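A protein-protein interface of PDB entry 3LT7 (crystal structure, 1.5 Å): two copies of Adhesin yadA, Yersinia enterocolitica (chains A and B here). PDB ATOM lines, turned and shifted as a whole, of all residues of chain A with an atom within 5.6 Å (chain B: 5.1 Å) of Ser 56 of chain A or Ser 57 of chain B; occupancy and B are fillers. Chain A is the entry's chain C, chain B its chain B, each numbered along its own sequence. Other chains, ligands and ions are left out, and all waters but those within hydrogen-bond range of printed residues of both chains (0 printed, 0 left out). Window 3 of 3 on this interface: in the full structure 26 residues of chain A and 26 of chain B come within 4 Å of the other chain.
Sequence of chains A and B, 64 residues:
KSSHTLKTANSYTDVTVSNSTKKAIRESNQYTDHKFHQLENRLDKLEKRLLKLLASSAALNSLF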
ATOM      1  N   LEU A  51     -35.371 -30.588 -21.163  1.00  0.00           N
ATOM      2  CA  LEU A  51     -34.263 -31.482 -20.813  1.00  0.00           C
ATOM      3  C   LEU A  51     -32.863 -30.849 -20.942  1.00  0.00           C
ATOM      4  O   LEU A  51     -31.990 -31.118 -20.121  1.00  0.00           O
ATOM      5  CB  LEU A  51     -34.344 -32.764 -21.633  1.00  0.00           C
ATOM      6  CG  LEU A  51     -35.286 -33.875 -21.159  1.00  0.00           C
ATOM      7  CD1 LEU A  51     -34.957 -35.140 -21.966  1.00  0.00           C
ATOM      8  CD2 LEU A  51     -35.227 -34.139 -19.653  1.00  0.00           C
ATOM      9  N   LYS A  52     -32.681 -29.999 -21.948  1.00  0.00           N
ATOM     10  CA  LYS A  52     -31.455 -29.208 -22.119  1.00  0.00           C
ATOM     11  C   LYS A  52     -31.392 -28.131 -21.020  1.00  0.00           C
ATOM     12  O   LYS A  52     -30.428 -28.062 -20.264  1.00  0.00           O
ATOM     13  CB  LYS A  52     -31.376 -28.591 -23.532  1.00  0.00           C
ATOM     14  CG  LYS A  52     -30.194 -27.600 -23.726  1.00  0.00           C
ATOM     15  CD  LYS A  52     -29.765 -27.445 -25.181  1.00  0.00           C
ATOM     16  CE  LYS A  52     -29.224 -26.030 -25.463  1.00  0.00           C
ATOM     17  NZ  LYS A  52     -28.374 -25.984 -26.682  1.00  0.00           N
ATOM     18  N   LEU A  53     -32.425 -27.298 -20.918  1.00  0.00           N
ATOM     19  CA  LEU A  53     -32.473 -26.281 -19.846  1.00  0.00           C
ATOM     20  C   LEU A  53     -32.149 -26.815 -18.438  1.00  0.00           C
ATOM     21  O   LEU A  53     -31.469 -26.132 -17.654  1.00  0.00           O
ATOM     22  CB  LEU A  53     -33.807 -25.518 -19.831  1.00  0.00           C
ATOM     23  CG  LEU A  53     -33.995 -24.605 -18.603  1.00  0.00           C
ATOM     24  CD1 LEU A  53     -33.180 -23.317 -18.755  1.00  0.00           C
ATOM     25  CD2 LEU A  53     -35.434 -24.306 -18.349  1.00  0.00           C
ATOM     26  N   LEU A  54     -32.634 -28.027 -18.134  1.00  0.00           N
ATOM     27  CA  LEU A  54     -32.428 -28.733 -16.866  1.00  0.00           C
ATOM     28  C   LEU A  54     -30.956 -29.011 -16.593  1.00  0.00           C
ATOM     29  O   LEU A  54     -30.467 -28.782 -15.483  1.00  0.00           O
ATOM     30  CB  LEU A  54     -33.088 -30.100 -16.919  1.00  0.00           C
ATOM     31  CG  LEU A  54     -34.245 -30.644 -16.093  1.00  0.00           C
ATOM     32  CD1 LEU A  54     -34.215 -32.141 -16.402  1.00  0.00           C
ATOM     33  CD2 LEU A  54     -34.114 -30.387 -14.605  1.00  0.00           C
ATOM     34  N   ALA A  55     -30.268 -29.539 -17.610  1.00  0.00           N
ATOM     35  CA  ALA A  55     -28.839 -29.867 -17.543  1.00  0.00           C
ATOM     36  C   ALA A  55     -28.004 -28.595 -17.522  1.00  0.00           C
ATOM     37  O   ALA A  55     -26.923 -28.554 -16.908  1.00  0.00           O
ATOM     38  CB  ALA A  55     -28.449 -30.716 -18.735  1.00  0.00           C
ATOM     39  N   SER A  56     -28.522 -27.569 -18.193  1.00  0.00           N
ATOM     40  CA  SER A  56     -27.926 -26.236 -18.207  1.00  0.00           C
ATOM     41  C   SER A  56     -27.960 -25.622 -16.806  1.00  0.00           C
ATOM     42  O   SER A  56     -26.977 -25.018 -16.363  1.00  0.00           O
ATOM     43  CB  SER A  56     -28.650 -25.329 -19.212  1.00  0.00           C
ATOM     44  OG  SER A  56     -28.032 -24.044 -19.279  1.00  0.00           O
ATOM     45  N   SER A  57     -29.081 -25.807 -16.107  1.00  0.00           N
ATOM     46  CA  SER A  57     -29.271 -25.242 -14.773  1.00  0.00           C
ATOM     47  C   SER A  57     -28.349 -25.836 -13.707  1.00  0.00           C
ATOM     48  O   SER A  57     -27.970 -25.143 -12.756  1.00  0.00           O
ATOM     49  CB  SER A  57     -30.722 -25.364 -14.324  1.00  0.00           C
ATOM     50  OG  SER A  57     -30.924 -24.704 -13.080  1.00  0.00           O
ATOM     51  N   ALA A  58     -28.020 -27.119 -13.840  1.00  0.00           N
ATOM     52  CA  ALA A  58     -27.119 -27.768 -12.899  1.00  0.00           C
ATOM     53  C   ALA A  58     -25.655 -27.597 -13.308  1.00  0.00           C
ATOM     54  O   ALA A  58     -24.747 -27.874 -12.523  1.00  0.00           O
ATOM     55  CB  ALA A  58     -27.475 -29.245 -12.738  1.00  0.00           C
ATOM     56  N   ALA A  59     -25.420 -27.157 -14.544  1.00  0.00           N
ATOM     57  CA  ALA A  59     -24.092 -26.673 -14.916  1.00  0.00           C
ATOM     58  C   ALA A  59     -23.792 -25.349 -14.196  1.00  0.00           C
ATOM     59  O   ALA A  59     -22.669 -25.162 -13.675  1.00  0.00           O
ATOM     60  CB  ALA A  59     -23.969 -26.518 -16.428  1.00  0.00           C
ATOM     61  N   LEU A  60     -24.811 -24.477 -14.114  1.00  0.00           N
ATOM     62  CA  LEU A  60     -24.723 -23.137 -13.483  1.00  0.00           C
ATOM     63  C   LEU A  60     -24.265 -23.145 -12.022  1.00  0.00           C
ATOM     64  O   LEU A  60     -23.626 -22.200 -11.561  1.00  0.00           O
ATOM     65  CB  LEU A  60     -26.030 -22.329 -13.636  1.00  0.00           C
ATOM     66  CG  LEU A  60     -26.073 -21.292 -14.776  1.00  0.00           C
ATOM     67  CD1 LEU A  60     -27.488 -20.944 -15.210  1.00  0.00           C
ATOM     68  CD2 LEU A  60     -25.296 -20.025 -14.427  1.00  0.00           C
ATOM     69  N   LEU B  53     -35.185 -18.622 -21.580  1.00  0.00           N
ATOM     70  CA  LEU B  53     -34.523 -19.157 -20.390  1.00  0.00           C
ATOM     71  C   LEU B  53     -33.240 -19.884 -20.747  1.00  0.00           C
ATOM     72  O   LEU B  53     -32.292 -19.891 -19.947  1.00  0.00           O
ATOM     73  CB  LEU B  53     -35.444 -20.100 -19.627  1.00  0.00           C
ATOM     74  CG  LEU B  53     -36.393 -19.496 -18.602  1.00  0.00           C
ATOM     75  CD1 LEU B  53     -37.389 -20.562 -18.239  1.00  0.00           C
ATOM     76  CD2 LEU B  53     -35.644 -18.986 -17.365  1.00  0.00           C
ATOM     77  N   LEU B  54     -33.223 -20.494 -21.935  1.00  0.00           N
ATOM     78  CA  LEU B  54     -32.010 -21.074 -22.484  1.00  0.00           C
ATOM     79  C   LEU B  54     -30.997 -20.005 -22.833  1.00  0.00           C
ATOM     80  O   LEU B  54     -29.797 -20.241 -22.682  1.00  0.00           O
ATOM     81  CB  LEU B  54     -32.301 -21.948 -23.711  1.00  0.00           C
ATOM     82  CG  LEU B  54     -32.777 -23.374 -23.442  1.00  0.00           C
ATOM     83  CD1 LEU B  54     -33.632 -23.868 -24.610  1.00  0.00           C
ATOM     84  CD2 LEU B  54     -31.602 -24.328 -23.149  1.00  0.00           C
ATOM     85  N   ALA B  55     -31.480 -18.852 -23.311  1.00  0.00           N
ATOM     86  CA  ALA B  55     -30.605 -17.743 -23.714  1.00  0.00           C
ATOM     87  C   ALA B  55     -29.929 -17.163 -22.491  1.00  0.00           C
ATOM     88  O   ALA B  55     -28.720 -16.938 -22.482  1.00  0.00           O
ATOM     89  CB  ALA B  55     -31.379 -16.666 -24.452  1.00  0.00           C
ATOM     90  N   SER B  56     -30.723 -16.925 -21.450  1.00  0.00           N
ATOM     91  CA  SER B  56     -30.194 -16.357 -20.227  1.00  0.00           C
ATOM     92  C   SER B  56     -29.232 -17.318 -19.521  1.00  0.00           C
ATOM     93  O   SER B  56     -28.117 -16.916 -19.221  1.00  0.00           O
ATOM     94  CB  SER B  56     -31.300 -15.846 -19.308  1.00  0.00           C
ATOM     95  OG  SER B  56     -32.386 -16.748 -19.278  1.00  0.00           O
ATOM     96  N   SER B  57     -29.651 -18.575 -19.294  1.00  0.00           N
ATOM     97  CA  SER B  57     -28.777 -19.638 -18.720  1.00  0.00           C
ATOM     98  C   SER B  57     -27.461 -19.902 -19.473  1.00  0.00           C
ATOM     99  O   SER B  57     -26.400 -20.068 -18.832  1.00  0.00           O
ATOM    100  CB  SER B  57     -29.535 -20.969 -18.510  1.00  0.00           C
ATOM    101  OG  SER B  57     -29.451 -21.849 -19.626  1.00  0.00           O
ATOM    102  N   ALA B  58     -27.527 -19.974 -20.809  1.00  0.00           N
ATOM    103  CA  ALA B  58     -26.317 -20.160 -21.617  1.00  0.00           C
ATOM    104  C   ALA B  58     -25.367 -18.978 -21.426  1.00  0.00           C
ATOM    105  O   ALA B  58     -24.185 -19.161 -21.106  1.00  0.00           O
ATOM    106  CB  ALA B  58     -26.658 -20.371 -23.101  1.00  0.00           C
ATOM    107  N   ALA B  59     -25.909 -17.766 -21.565  1.00  0.00           N
ATOM    108  CA  ALA B  59     -25.133 -16.539 -21.365  1.00  0.00           C
ATOM    109  C   ALA B  59     -24.538 -16.445 -19.958  1.00  0.00           C
ATOM    110  O   ALA B  59     -23.387 -16.029 -19.792  1.00  0.00           O
ATOM    111  CB  ALA B  59     -25.974 -15.318 -21.685  1.00  0.00           C
ATOM    112  N   LEU B  60     -25.312 -16.856 -18.953  1.00  0.00           N
ATOM    113  CA  LEU B  60     -24.825 -16.924 -17.580  1.00  0.00           C
ATOM    114  C   LEU B  60     -23.692 -17.956 -17.431  1.00  0.00           C
ATOM    115  O   LEU B  60     -22.726 -17.723 -16.695  1.00  0.00           O
ATOM    116  CB  LEU B  60     -25.973 -17.240 -16.629  1.00  0.00           C
ATOM    117  CG  LEU B  60     -26.127 -16.350 -15.385  1.00  0.00           C
ATOM    118  CD1 LEU B  60     -27.161 -16.918 -14.412  1.00  0.00           C
ATOM    119  CD2 LEU B  60     -24.804 -16.135 -14.675  1.00  0.00           C
ATOM    120  N   ASN B  61     -23.811 -19.078 -18.146  1.00  0.00           N
ATOM    121  CA  ASN B  61     -22.769 -20.120 -18.155  1.00  0.00           C
ATOM    122  C   ASN B  61     -21.444 -19.691 -18.790  1.00  0.00           C
ATOM    123  O   ASN B  61     -20.384 -19.876 -18.177  1.00  0.00           O
ATOM    124  CB  ASN B  61     -23.277 -21.428 -18.775  1.00  0.00           C
ATOM    125  CG  ASN B  61     -23.860 -22.390 -17.740  1.00  0.00           C
ATOM    126  OD1 ASN B  61     -23.146 -22.884 -16.859  1.00  0.00           O
ATOM    127  ND2 ASN B  61     -25.153 -22.681 -17.861  1.00  0.00           N
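O of Leu 53 of chain B is in hydrogen-bond range of OG of Ser 56 of chain B, 3.2 Å away.
O of Leu 53 of chain B sits close to OG of Ser 57 of chain B.
The side-chain hydroxyl (OG) of Ser 57 of chain B sits at hydrogen-bond distance from the backbone carbonyl oxygen (O) of Leu 54 of chain B, at 3.5 Å.
O of Ser 57 of chain B lies within hydrogen-bond range of ND2 of Asn 61 of chain B (3.1 Å).
The side-chain hydroxyl (OG) of Ser 57 of chain B lies within hydrogen-bond range of the side-chain hydroxyl (OG) of Ser 56 of chain A (2.6 Å).
ND2 of Asn 61 of chain B sits at hydrogen-bond distance from O of Ser 56 of chain A (3.3 Å).
Hydrophobic or aromatic side chains of chain A within 4 Å of the printed part of chain B: Leu 53, Ala 59 and Leu 60.
Of the 9 printed residues of chain B, 5 touch a printed residue of chain A.
Printed residues of chain B that touch a printed residue of chain A: Leu 53, Leu 54, Ser 57, Leu 60 and Asn 61.
Among the printed residues, no Asp or Glu carboxylate lies within 4 Å of a Lys or Arg side-chain nitrogen of the other chain.
Leu 54 of chain B touches Lys 52 of chain A (CD2 to CG, 3.6 Å).
O of Leu 53 of chain B touches CD1 of Leu 53 of chain A, at 3.7 Å.
Leu 54 of chain B touches Leu 53 of chain A.
C of Ala 59 of chain A touches OD1 of Asn 61 of chain B, 3.7 Å away.
O of Ser 57 of chain B touches CD1 of Leu 60 of chain A, at 3.9 Å.
Leu 60 of chain B touches Leu 60 of chain A (CB to CD2, 3.6 Å).
Asn 61 of chain B touches Leu 60 of chain A (ND2 to CG, 3.5 Å).
Ser 56 of chain A touches just these residues of chain B: Ser 57 and Asn 61.
Printed residues of chain A within 4 Å of Ser 57 of chain B: Ser 56 (2.6 Å) and Leu 60 (3.9 Å).
Of the printed residues of chain B, Leu 53 of chain A touches Leu 53 and Leu 54.
Of the printed residues of chain B, Ala 59 of chain A touches Asn 61.
Of the printed residues of chain A, Leu 60 of chain B touches Leu 60.
Of the printed residues of chain A, Leu 54 of chain B touches Lys 52 and Leu 53.
Printed residues of chain B within 4 Å of Lys 52 of chain A: Leu 54.
Ser 56 of chain B touches none of the printed residues of chain A.
The nearest residue of chain B that does not touch Ser 56 of chain A is Ala 58 of chain B (4.4 Å).
The nearest printed residue of chain A that does not touch Leu 54 of chain B is Ser 56 of chain A (5.0 Å).
Leu 53 of chain B touches its own counterpart, Leu 53 of chain A.
Leu 53 of chain A touches Leu 54 of chain B, but with the chains exchanged Leu 54 of chain A does not touch Leu 53 of chain B (8.3 Å).
Leu 60 of chain A touches Ser 57 of chain B, but with the chains exchanged Ser 57 of chain A does not touch Leu 60 of chain B (8.4 Å).
Leu 60 of chain A touches its own counterpart, Leu 60 of chain B.
8 positions are printed for both chains.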
